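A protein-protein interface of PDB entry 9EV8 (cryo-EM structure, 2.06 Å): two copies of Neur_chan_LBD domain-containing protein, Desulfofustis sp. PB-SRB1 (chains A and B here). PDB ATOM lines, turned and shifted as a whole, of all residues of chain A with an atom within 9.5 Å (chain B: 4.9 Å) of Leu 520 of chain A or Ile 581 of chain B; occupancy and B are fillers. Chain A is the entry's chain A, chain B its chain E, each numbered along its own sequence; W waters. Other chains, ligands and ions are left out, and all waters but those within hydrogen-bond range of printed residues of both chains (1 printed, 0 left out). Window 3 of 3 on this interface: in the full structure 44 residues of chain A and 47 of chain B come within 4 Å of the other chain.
OE2 of Glu 516 of chain A is in salt-bridge range of NH1 of Arg 578 of chain B, at 3.7 Å.
The backbone carbonyl oxygen of Ile 581 of chain B is in hydrogen-bond range of the side-chain sulfur of Cys 585 of chain B, 3.2 Å away.
Among the printed residues, merely in contact across the chains: Glu 516 of chain A with Leu 573 of chain B, Leu 520 of chain A with Leu 573 of chain B, Leu 520 of chain A with Ile 581 of chain B, Pro 525 of chain A with Phe 584 of chain B and Leu 528 of chain A with Cys 585 of chain B.
Of the printed residues of chain B, Glu 516 of chain A touches Leu 573 (3.9 Å) and Arg 578 (3.7 Å).
Tyr 518 of chain A touches none of the printed residues of chain B.
Arg 521 of chain A touches none of the printed residues of chain B.
Printed residues of chain B within 4 Å of Pro 525 of chain A: Phe 584 (3.9 Å).
Of the printed residues of chain B, Leu 528 of chain A touches Cys 585 (3.9 Å).
Of the printed residues of chain A, Arg 578 of chain B touches Glu 516.
Of chain A, only Leu 520 (3.5 Å) comes within 4 Å of Ile 581 of chain B.
Val 582 of chain B touches none of the printed residues of chain A.
Of the printed residues of chain A, Phe 584 of chain B touches Pro 525 (3.9 Å).
The nearest printed residue of chain B that does not touch Leu 520 of chain A is Arg 578 of chain B (4.9 Å).
Printed residues of chain A that touch a printed residue of chain B: Glu 516, Leu 520, Pro 525 and Leu 528.
Hydrophobic or aromatic side chains of chain A that line the printed part of chain B: Leu 520, Pro 525 and Leu 528.
Of the 10 printed residues of chain B, 5 touch a printed residue of chain A.
Printed residues of chain B that touch a printed residue of chain A: Leu 573, Arg 578, Ile 581, Phe 584 and Cys 585.
Hydrophobic or aromatic side chains of chain B within 4 Å of the printed part of chain A: Leu 573, Ile 581 and Phe 584.
Among the printed residues, 6 pairs touch across the chains.
No position is printed for both chains.
Of the 6 pairs that touch across the chains among the printed residues, none has its exchanged pair printed and touching as well.
Water W1 lies within hydrogen-bond range of OD1 of Asn 514 of chain A (3.0 Å), N of Leu 573 of chain B (3.2 Å) and OE1 of Glu 516 of chain A (3.4 Å).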
ATOM      1  N   ASN A 514     -19.676 -24.480   9.224  1.00  0.00           N
ATOM      2  CA  ASN A 514     -20.485 -25.503   8.566  1.00  0.00           C
ATOM      3  C   ASN A 514     -19.572 -26.436   7.780  1.00  0.00           C
ATOM      4  O   ASN A 514     -18.951 -26.027   6.794  1.00  0.00           O
ATOM      5  CB  ASN A 514     -21.520 -24.846   7.659  1.00  0.00           C
ATOM      6  CG  ASN A 514     -22.492 -25.841   7.062  1.00  0.00           C
ATOM      7  OD1 ASN A 514     -22.257 -26.384   5.984  1.00  0.00           O
ATOM      8  ND2 ASN A 514     -23.593 -26.084   7.762  1.00  0.00           N
ATOM      9  N   LEU A 515     -19.486 -27.693   8.217  1.00  0.00           N
ATOM     10  CA  LEU A 515     -18.523 -28.629   7.645  1.00  0.00           C
ATOM     11  C   LEU A 515     -18.967 -29.174   6.290  1.00  0.00           C
ATOM     12  O   LEU A 515     -18.121 -29.423   5.421  1.00  0.00           O
ATOM     13  CB  LEU A 515     -18.283 -29.779   8.622  1.00  0.00           C
ATOM     14  CG  LEU A 515     -16.868 -30.351   8.668  1.00  0.00           C
ATOM     15  CD1 LEU A 515     -15.897 -29.306   9.189  1.00  0.00           C
ATOM     16  CD2 LEU A 515     -16.822 -31.606   9.523  1.00  0.00           C
ATOM     17  N   GLU A 516     -20.275 -29.368   6.100  1.00  0.00           N
ATOM     18  CA  GLU A 516     -20.777 -29.922   4.846  1.00  0.00           C
ATOM     19  C   GLU A 516     -20.397 -29.045   3.662  1.00  0.00           C
ATOM     20  O   GLU A 516     -20.044 -29.549   2.591  1.00  0.00           O
ATOM     21  CB  GLU A 516     -22.296 -30.086   4.917  1.00  0.00           C
ATOM     22  CG  GLU A 516     -22.929 -30.594   3.633  1.00  0.00           C
ATOM     23  CD  GLU A 516     -24.444 -30.513   3.655  1.00  0.00           C
ATOM     24  OE1 GLU A 516     -24.995 -29.881   4.580  1.00  0.00           O
ATOM     25  OE2 GLU A 516     -25.084 -31.081   2.745  1.00  0.00           O
ATOM     26  N   TYR A 517     -20.464 -27.725   3.845  1.00  0.00           N
ATOM     27  CA  TYR A 517     -20.110 -26.794   2.783  1.00  0.00           C
ATOM     28  C   TYR A 517     -18.699 -27.053   2.271  1.00  0.00           C
ATOM     29  O   TYR A 517     -18.497 -27.304   1.077  1.00  0.00           O
ATOM     30  CB  TYR A 517     -20.253 -25.364   3.313  1.00  0.00           C
ATOM     31  CG  TYR A 517     -19.803 -24.267   2.381  1.00  0.00           C
ATOM     32  CD1 TYR A 517     -20.605 -23.849   1.331  1.00  0.00           C
ATOM     33  CD2 TYR A 517     -18.589 -23.623   2.575  1.00  0.00           C
ATOM     34  CE1 TYR A 517     -20.206 -22.836   0.489  1.00  0.00           C
ATOM     35  CE2 TYR A 517     -18.179 -22.608   1.735  1.00  0.00           C
ATOM     36  CZ  TYR A 517     -18.994 -22.218   0.693  1.00  0.00           C
ATOM     37  OH  TYR A 517     -18.599 -21.208  -0.152  1.00  0.00           O
ATOM     38  N   TYR A 518     -17.718 -27.064   3.177  1.00  0.00           N
ATOM     39  CA  TYR A 518     -16.334 -27.271   2.770  1.00  0.00           C
ATOM     40  C   TYR A 518     -16.121 -28.669   2.208  1.00  0.00           C
ATOM     41  O   TYR A 518     -15.478 -28.828   1.162  1.00  0.00           O
ATOM     42  CB  TYR A 518     -15.391 -27.016   3.945  1.00  0.00           C
ATOM     43  CG  TYR A 518     -15.287 -25.561   4.321  1.00  0.00           C
ATOM     44  CD1 TYR A 518     -14.471 -24.698   3.608  1.00  0.00           C
ATOM     45  CD2 TYR A 518     -16.011 -25.049   5.385  1.00  0.00           C
ATOM     46  CE1 TYR A 518     -14.380 -23.366   3.945  1.00  0.00           C
ATOM     47  CE2 TYR A 518     -15.926 -23.721   5.730  1.00  0.00           C
ATOM     48  CZ  TYR A 518     -15.110 -22.882   5.008  1.00  0.00           C
ATOM     49  OH  TYR A 518     -15.025 -21.555   5.354  1.00  0.00           O
ATOM     50  N   ILE A 519     -16.672 -29.693   2.866  1.00  0.00           N
ATOM     51  CA  ILE A 519     -16.460 -31.063   2.408  1.00  0.00           C
ATOM     52  C   ILE A 519     -16.964 -31.230   0.980  1.00  0.00           C
ATOM     53  O   ILE A 519     -16.190 -31.563   0.073  1.00  0.00           O
ATOM     54  CB  ILE A 519     -17.135 -32.061   3.367  1.00  0.00           C
ATOM     55  CG1 ILE A 519     -16.382 -32.119   4.695  1.00  0.00           C
ATOM     56  CG2 ILE A 519     -17.201 -33.441   2.743  1.00  0.00           C
ATOM     57  CD1 ILE A 519     -17.003 -33.057   5.702  1.00  0.00           C
ATOM     58  N   LEU A 520     -18.239 -30.910   0.745  1.00  0.00           N
ATOM     59  CA  LEU A 520     -18.828 -31.119  -0.571  1.00  0.00           C
ATOM     60  C   LEU A 520     -18.218 -30.197  -1.619  1.00  0.00           C
ATOM     61  O   LEU A 520     -18.091 -30.585  -2.785  1.00  0.00           O
ATOM     62  CB  LEU A 520     -20.342 -30.920  -0.502  1.00  0.00           C
ATOM     63  CG  LEU A 520     -21.208 -32.167  -0.314  1.00  0.00           C
ATOM     64  CD1 LEU A 520     -20.712 -33.026   0.833  1.00  0.00           C
ATOM     65  CD2 LEU A 520     -22.657 -31.769  -0.093  1.00  0.00           C
ATOM     66  N   ARG A 521     -17.825 -28.978  -1.235  1.00  0.00           N
ATOM     67  CA  ARG A 521     -17.349 -28.028  -2.231  1.00  0.00           C
ATOM     68  C   ARG A 521     -15.900 -28.283  -2.634  1.00  0.00           C
ATOM     69  O   ARG A 521     -15.521 -27.998  -3.776  1.00  0.00           O
ATOM     70  CB  ARG A 521     -17.521 -26.601  -1.708  1.00  0.00           C
ATOM     71  CG  ARG A 521     -17.171 -25.518  -2.712  1.00  0.00           C
ATOM     72  CD  ARG A 521     -17.553 -24.138  -2.200  1.00  0.00           C
ATOM     73  NE  ARG A 521     -16.850 -23.080  -2.918  1.00  0.00           N
ATOM     74  CZ  ARG A 521     -17.236 -22.577  -4.083  1.00  0.00           C
ATOM     75  NH1 ARG A 521     -18.322 -23.015  -4.698  1.00  0.00           N
ATOM     76  NH2 ARG A 521     -16.512 -21.612  -4.645  1.00  0.00           N
ATOM     77  N   ILE A 522     -15.071 -28.814  -1.738  1.00  0.00           N
ATOM     78  CA  ILE A 522     -13.635 -28.933  -1.983  1.00  0.00           C
ATOM     79  C   ILE A 522     -13.191 -30.392  -2.087  1.00  0.00           C
ATOM     80  O   ILE A 522     -12.563 -30.787  -3.071  1.00  0.00           O
ATOM     81  CB  ILE A 522     -12.823 -28.172  -0.911  1.00  0.00           C
ATOM     82  CG1 ILE A 522     -13.161 -26.681  -0.961  1.00  0.00           C
ATOM     83  CG2 ILE A 522     -11.335 -28.381  -1.120  1.00  0.00           C
ATOM     84  CD1 ILE A 522     -12.408 -25.849   0.051  1.00  0.00           C
ATOM     85  N   PHE A 523     -13.496 -31.209  -1.073  1.00  0.00           N
ATOM     86  CA  PHE A 523     -12.748 -32.454  -0.909  1.00  0.00           C
ATOM     87  C   PHE A 523     -13.160 -33.521  -1.919  1.00  0.00           C
ATOM     88  O   PHE A 523     -12.304 -34.251  -2.432  1.00  0.00           O
ATOM     89  CB  PHE A 523     -12.896 -32.961   0.525  1.00  0.00           C
ATOM     90  CG  PHE A 523     -12.184 -32.107   1.535  1.00  0.00           C
ATOM     91  CD1 PHE A 523     -10.802 -32.079   1.585  1.00  0.00           C
ATOM     92  CD2 PHE A 523     -12.896 -31.324   2.425  1.00  0.00           C
ATOM     93  CE1 PHE A 523     -10.142 -31.290   2.508  1.00  0.00           C
ATOM     94  CE2 PHE A 523     -12.242 -30.533   3.350  1.00  0.00           C
ATOM     95  CZ  PHE A 523     -10.866 -30.516   3.392  1.00  0.00           C
ATOM     96  N   VAL A 524     -14.456 -33.640  -2.216  1.00  0.00           N
ATOM     97  CA  VAL A 524     -14.900 -34.645  -3.185  1.00  0.00           C
ATOM     98  C   VAL A 524     -14.347 -34.384  -4.583  1.00  0.00           C
ATOM     99  O   VAL A 524     -13.794 -35.320  -5.191  1.00  0.00           O
ATOM    100  CB  VAL A 524     -16.438 -34.760  -3.157  1.00  0.00           C
ATOM    101  CG1 VAL A 524     -16.922 -35.756  -4.196  1.00  0.00           C
ATOM    102  CG2 VAL A 524     -16.912 -35.156  -1.771  1.00  0.00           C
ATOM    103  N   PRO A 525     -14.450 -33.172  -5.153  1.00  0.00           N
ATOM    104  CA  PRO A 525     -13.812 -32.942  -6.460  1.00  0.00           C
ATOM    105  C   PRO A 525     -12.315 -33.193  -6.452  1.00  0.00           C
ATOM    106  O   PRO A 525     -11.769 -33.719  -7.430  1.00  0.00           O
ATOM    107  CB  PRO A 525     -14.141 -31.469  -6.752  1.00  0.00           C
ATOM    108  CG  PRO A 525     -15.362 -31.194  -5.967  1.00  0.00           C
ATOM    109  CD  PRO A 525     -15.212 -31.989  -4.712  1.00  0.00           C
ATOM    110  N   LEU A 526     -11.636 -32.833  -5.361  1.00  0.00           N
ATOM    111  CA  LEU A 526     -10.204 -33.093  -5.255  1.00  0.00           C
ATOM    112  C   LEU A 526      -9.917 -34.588  -5.278  1.00  0.00           C
ATOM    113  O   LEU A 526      -8.960 -35.038  -5.922  1.00  0.00           O
ATOM    114  CB  LEU A 526      -9.659 -32.451  -3.980  1.00  0.00           C
ATOM    115  CG  LEU A 526      -8.166 -32.138  -3.920  1.00  0.00           C
ATOM    116  CD1 LEU A 526      -7.780 -31.213  -5.056  1.00  0.00           C
ATOM    117  CD2 LEU A 526      -7.817 -31.515  -2.583  1.00  0.00           C
ATOM    118  N   PHE A 527     -10.742 -35.376  -4.585  1.00  0.00           N
ATOM    119  CA  PHE A 527     -10.578 -36.825  -4.604  1.00  0.00           C
ATOM    120  C   PHE A 527     -10.760 -37.386  -6.009  1.00  0.00           C
ATOM    121  O   PHE A 527     -10.001 -38.264  -6.435  1.00  0.00           O
ATOM    122  CB  PHE A 527     -11.561 -37.476  -3.628  1.00  0.00           C
ATOM    123  CG  PHE A 527     -11.540 -38.977  -3.657  1.00  0.00           C
ATOM    124  CD1 PHE A 527     -10.544 -39.680  -3.001  1.00  0.00           C
ATOM    125  CD2 PHE A 527     -12.512 -39.685  -4.343  1.00  0.00           C
ATOM    126  CE1 PHE A 527     -10.520 -41.059  -3.029  1.00  0.00           C
ATOM    127  CE2 PHE A 527     -12.491 -41.063  -4.375  1.00  0.00           C
ATOM    128  CZ  PHE A 527     -11.494 -41.750  -3.717  1.00  0.00           C
ATOM    129  N   LEU A 528     -11.759 -36.895  -6.746  1.00  0.00           N
ATOM    130  CA  LEU A 528     -11.963 -37.374  -8.113  1.00  0.00           C
ATOM    131  C   LEU A 528     -10.787 -37.005  -9.018  1.00  0.00           C
ATOM    132  O   LEU A 528     -10.356 -37.805  -9.860  1.00  0.00           O
ATOM    133  CB  LEU A 528     -13.278 -36.827  -8.668  1.00  0.00           C
ATOM    134  CG  LEU A 528     -14.529 -37.422  -8.020  1.00  0.00           C
ATOM    135  CD1 LEU A 528     -15.785 -36.778  -8.565  1.00  0.00           C
ATOM    136  CD2 LEU A 528     -14.568 -38.928  -8.219  1.00  0.00           C
ATOM    137  N   PHE A 559      -8.821 -26.014 -11.076  1.00  0.00           N
ATOM    138  CA  PHE A 559      -9.703 -26.174  -9.922  1.00  0.00           C
ATOM    139  C   PHE A 559      -9.168 -25.425  -8.709  1.00  0.00           C
ATOM    140  O   PHE A 559      -9.938 -24.823  -7.946  1.00  0.00           O
ATOM    141  CB  PHE A 559      -9.887 -27.655  -9.596  1.00  0.00           C
ATOM    142  CG  PHE A 559     -10.653 -27.905  -8.327  1.00  0.00           C
ATOM    143  CD1 PHE A 559     -12.034 -27.859  -8.318  1.00  0.00           C
ATOM    144  CD2 PHE A 559      -9.989 -28.184  -7.144  1.00  0.00           C
ATOM    145  CE1 PHE A 559     -12.738 -28.087  -7.155  1.00  0.00           C
ATOM    146  CE2 PHE A 559     -10.690 -28.411  -5.979  1.00  0.00           C
ATOM    147  CZ  PHE A 559     -12.066 -28.366  -5.985  1.00  0.00           C
ATOM    148  N   ILE A 563     -11.223 -22.501  -6.623  1.00  0.00           N
ATOM    149  CA  ILE A 563     -11.583 -22.508  -5.208  1.00  0.00           C
ATOM    150  C   ILE A 563     -10.745 -21.519  -4.408  1.00  0.00           C
ATOM    151  O   ILE A 563     -10.922 -21.406  -3.191  1.00  0.00           O
ATOM    152  CB  ILE A 563     -11.478 -23.916  -4.599  1.00  0.00           C
ATOM    153  CG1 ILE A 563     -10.012 -24.333  -4.467  1.00  0.00           C
ATOM    154  CG2 ILE A 563     -12.266 -24.914  -5.434  1.00  0.00           C
ATOM    155  CD1 ILE A 563      -9.809 -25.658  -3.776  1.00  0.00           C
ATOM    156  N   ASP A 566     -12.291 -19.471  -1.466  1.00  0.00           N
ATOM    157  CA  ASP A 566     -12.458 -19.986  -0.113  1.00  0.00           C
ATOM    158  C   ASP A 566     -11.123 -20.245   0.574  1.00  0.00           C
ATOM    159  O   ASP A 566     -11.045 -21.099   1.463  1.00  0.00           O
ATOM    160  CB  ASP A 566     -13.299 -21.264  -0.128  1.00  0.00           C
ATOM    161  CG  ASP A 566     -14.716 -21.025  -0.614  1.00  0.00           C
ATOM    162  OD1 ASP A 566     -15.238 -19.911  -0.399  1.00  0.00           O
ATOM    163  OD2 ASP A 566     -15.305 -21.951  -1.213  1.00  0.00           O
ATOM    164  N   LEU B 573     -24.574 -24.386   1.619  1.00  0.00           N
ATOM    165  CA  LEU B 573     -24.896 -24.792   0.258  1.00  0.00           C
ATOM    166  C   LEU B 573     -26.258 -24.272  -0.183  1.00  0.00           C
ATOM    167  O   LEU B 573     -27.221 -24.285   0.588  1.00  0.00           O
ATOM    168  CB  LEU B 573     -24.860 -26.315   0.140  1.00  0.00           C
ATOM    169  CG  LEU B 573     -23.489 -26.983   0.239  1.00  0.00           C
ATOM    170  CD1 LEU B 573     -23.627 -28.494   0.263  1.00  0.00           C
ATOM    171  CD2 LEU B 573     -22.605 -26.545  -0.914  1.00  0.00           C
ATOM    172  N   ASP B 577     -25.203 -24.620  -6.087  1.00  0.00           N
ATOM    173  CA  ASP B 577     -23.960 -25.299  -5.728  1.00  0.00           C
ATOM    174  C   ASP B 577     -24.120 -26.813  -5.810  1.00  0.00           C
ATOM    175  O   ASP B 577     -23.239 -27.516  -6.322  1.00  0.00           O
ATOM    176  CB  ASP B 577     -23.521 -24.881  -4.324  1.00  0.00           C
ATOM    177  CG  ASP B 577     -23.344 -23.383  -4.192  1.00  0.00           C
ATOM    178  OD1 ASP B 577     -23.071 -22.724  -5.214  1.00  0.00           O
ATOM    179  OD2 ASP B 577     -23.470 -22.866  -3.062  1.00  0.00           O
ATOM    180  N   ARG B 578     -25.240 -27.332  -5.304  1.00  0.00           N
ATOM    181  CA  ARG B 578     -25.487 -28.768  -5.367  1.00  0.00           C
ATOM    182  C   ARG B 578     -25.564 -29.251  -6.807  1.00  0.00           C
ATOM    183  O   ARG B 578     -24.994 -30.298  -7.155  1.00  0.00           O
ATOM    184  CB  ARG B 578     -26.772 -29.106  -4.614  1.00  0.00           C
ATOM    185  CG  ARG B 578     -26.751 -28.714  -3.149  1.00  0.00           C
ATOM    186  CD  ARG B 578     -28.085 -28.982  -2.479  1.00  0.00           C
ATOM    187  NE  ARG B 578     -28.118 -28.483  -1.109  1.00  0.00           N
ATOM    188  CZ  ARG B 578     -27.747 -29.184  -0.045  1.00  0.00           C
ATOM    189  NH1 ARG B 578     -27.319 -30.429  -0.152  1.00  0.00           N
ATOM    190  NH2 ARG B 578     -27.801 -28.615   1.155  1.00  0.00           N
ATOM    191  N   PHE B 579     -26.258 -28.499  -7.667  1.00  0.00           N
ATOM    192  CA  PHE B 579     -26.347 -28.902  -9.068  1.00  0.00           C
ATOM    193  C   PHE B 579     -24.974 -28.895  -9.738  1.00  0.00           C
ATOM    194  O   PHE B 579     -24.647 -29.814 -10.501  1.00  0.00           O
ATOM    195  CB  PHE B 579     -27.324 -28.001  -9.823  1.00  0.00           C
ATOM    196  CG  PHE B 579     -27.756 -28.565 -11.145  1.00  0.00           C
ATOM    197  CD1 PHE B 579     -28.795 -29.476 -11.216  1.00  0.00           C
ATOM    198  CD2 PHE B 579     -27.114 -28.197 -12.314  1.00  0.00           C
ATOM    199  CE1 PHE B 579     -29.191 -30.005 -12.427  1.00  0.00           C
ATOM    200  CE2 PHE B 579     -27.506 -28.724 -13.528  1.00  0.00           C
ATOM    201  CZ  PHE B 579     -28.545 -29.627 -13.586  1.00  0.00           C
ATOM    202  N   MET B 580     -24.159 -27.874  -9.458  1.00  0.00           N
ATOM    203  CA  MET B 580     -22.817 -27.819 -10.035  1.00  0.00           C
ATOM    204  C   MET B 580     -21.971 -29.005  -9.584  1.00  0.00           C
ATOM    205  O   MET B 580     -21.256 -29.609 -10.394  1.00  0.00           O
ATOM    206  CB  MET B 580     -22.135 -26.503  -9.660  1.00  0.00           C
ATOM    207  CG  MET B 580     -22.803 -25.256 -10.220  1.00  0.00           C
ATOM    208  SD  MET B 580     -22.869 -25.204 -12.022  1.00  0.00           S
ATOM    209  CE  MET B 580     -21.127 -25.159 -12.429  1.00  0.00           C
ATOM    210  N   ILE B 581     -22.043 -29.351  -8.296  1.00  0.00           N
ATOM    211  CA  ILE B 581     -21.269 -30.484  -7.793  1.00  0.00           C
ATOM    212  C   ILE B 581     -21.693 -31.788  -8.459  1.00  0.00           C
ATOM    213  O   ILE B 581     -20.840 -32.586  -8.876  1.00  0.00           O
ATOM    214  CB  ILE B 581     -21.419 -30.599  -6.264  1.00  0.00           C
ATOM    215  CG1 ILE B 581     -20.786 -29.392  -5.573  1.00  0.00           C
ATOM    216  CG2 ILE B 581     -20.796 -31.894  -5.765  1.00  0.00           C
ATOM    217  CD1 ILE B 581     -21.112 -29.291  -4.100  1.00  0.00           C
ATOM    218  N   VAL B 582     -23.005 -32.018  -8.581  1.00  0.00           N
ATOM    219  CA  VAL B 582     -23.484 -33.248  -9.209  1.00  0.00           C
ATOM    220  C   VAL B 582     -23.035 -33.319 -10.664  1.00  0.00           C
ATOM    221  O   VAL B 582     -22.585 -34.373 -11.146  1.00  0.00           O
ATOM    222  CB  VAL B 582     -25.017 -33.353  -9.077  1.00  0.00           C
ATOM    223  CG1 VAL B 582     -25.553 -34.501  -9.915  1.00  0.00           C
ATOM    224  CG2 VAL B 582     -25.412 -33.533  -7.624  1.00  0.00           C
ATOM    225  N   SER B 583     -23.139 -32.201 -11.388  1.00  0.00           N
ATOM    226  CA  SER B 583     -22.737 -32.186 -12.790  1.00  0.00           C
ATOM    227  C   SER B 583     -21.243 -32.467 -12.946  1.00  0.00           C
ATOM    228  O   SER B 583     -20.841 -33.231 -13.833  1.00  0.00           O
ATOM    229  CB  SER B 583     -23.110 -30.847 -13.423  1.00  0.00           C
ATOM    230  OG  SER B 583     -22.891 -30.865 -14.823  1.00  0.00           O
ATOM    231  N   PHE B 584     -20.409 -31.868 -12.091  1.00  0.00           N
ATOM    232  CA  PHE B 584     -18.973 -32.133 -12.154  1.00  0.00           C
ATOM    233  C   PHE B 584     -18.672 -33.604 -11.885  1.00  0.00           C
ATOM    234  O   PHE B 584     -17.837 -34.218 -12.565  1.00  0.00           O
ATOM    235  CB  PHE B 584     -18.223 -31.246 -11.158  1.00  0.00           C
ATOM    236  CG  PHE B 584     -16.727 -31.420 -11.199  1.00  0.00           C
ATOM    237  CD1 PHE B 584     -16.103 -32.390 -10.433  1.00  0.00           C
ATOM    238  CD2 PHE B 584     -15.946 -30.616 -12.008  1.00  0.00           C
ATOM    239  CE1 PHE B 584     -14.733 -32.556 -10.479  1.00  0.00           C
ATOM    240  CE2 PHE B 584     -14.577 -30.775 -12.053  1.00  0.00           C
ATOM    241  CZ  PHE B 584     -13.971 -31.745 -11.287  1.00  0.00           C
ATOM    242  N   CYS B 585     -19.331 -34.182 -10.876  1.00  0.00           N
ATOM    243  CA  CYS B 585     -19.082 -35.581 -10.546  1.00  0.00           C
ATOM    244  C   CYS B 585     -19.433 -36.492 -11.717  1.00  0.00           C
ATOM    245  O   CYS B 585     -18.671 -37.404 -12.064  1.00  0.00           O
ATOM    246  CB  CYS B 585     -19.869 -35.972  -9.296  1.00  0.00           C
ATOM    247  SG  CYS B 585     -19.301 -35.165  -7.782  1.00  0.00           S
HETATM  248  O   HOH W   1     -24.179 -26.715   3.743  1.00  0.00           O
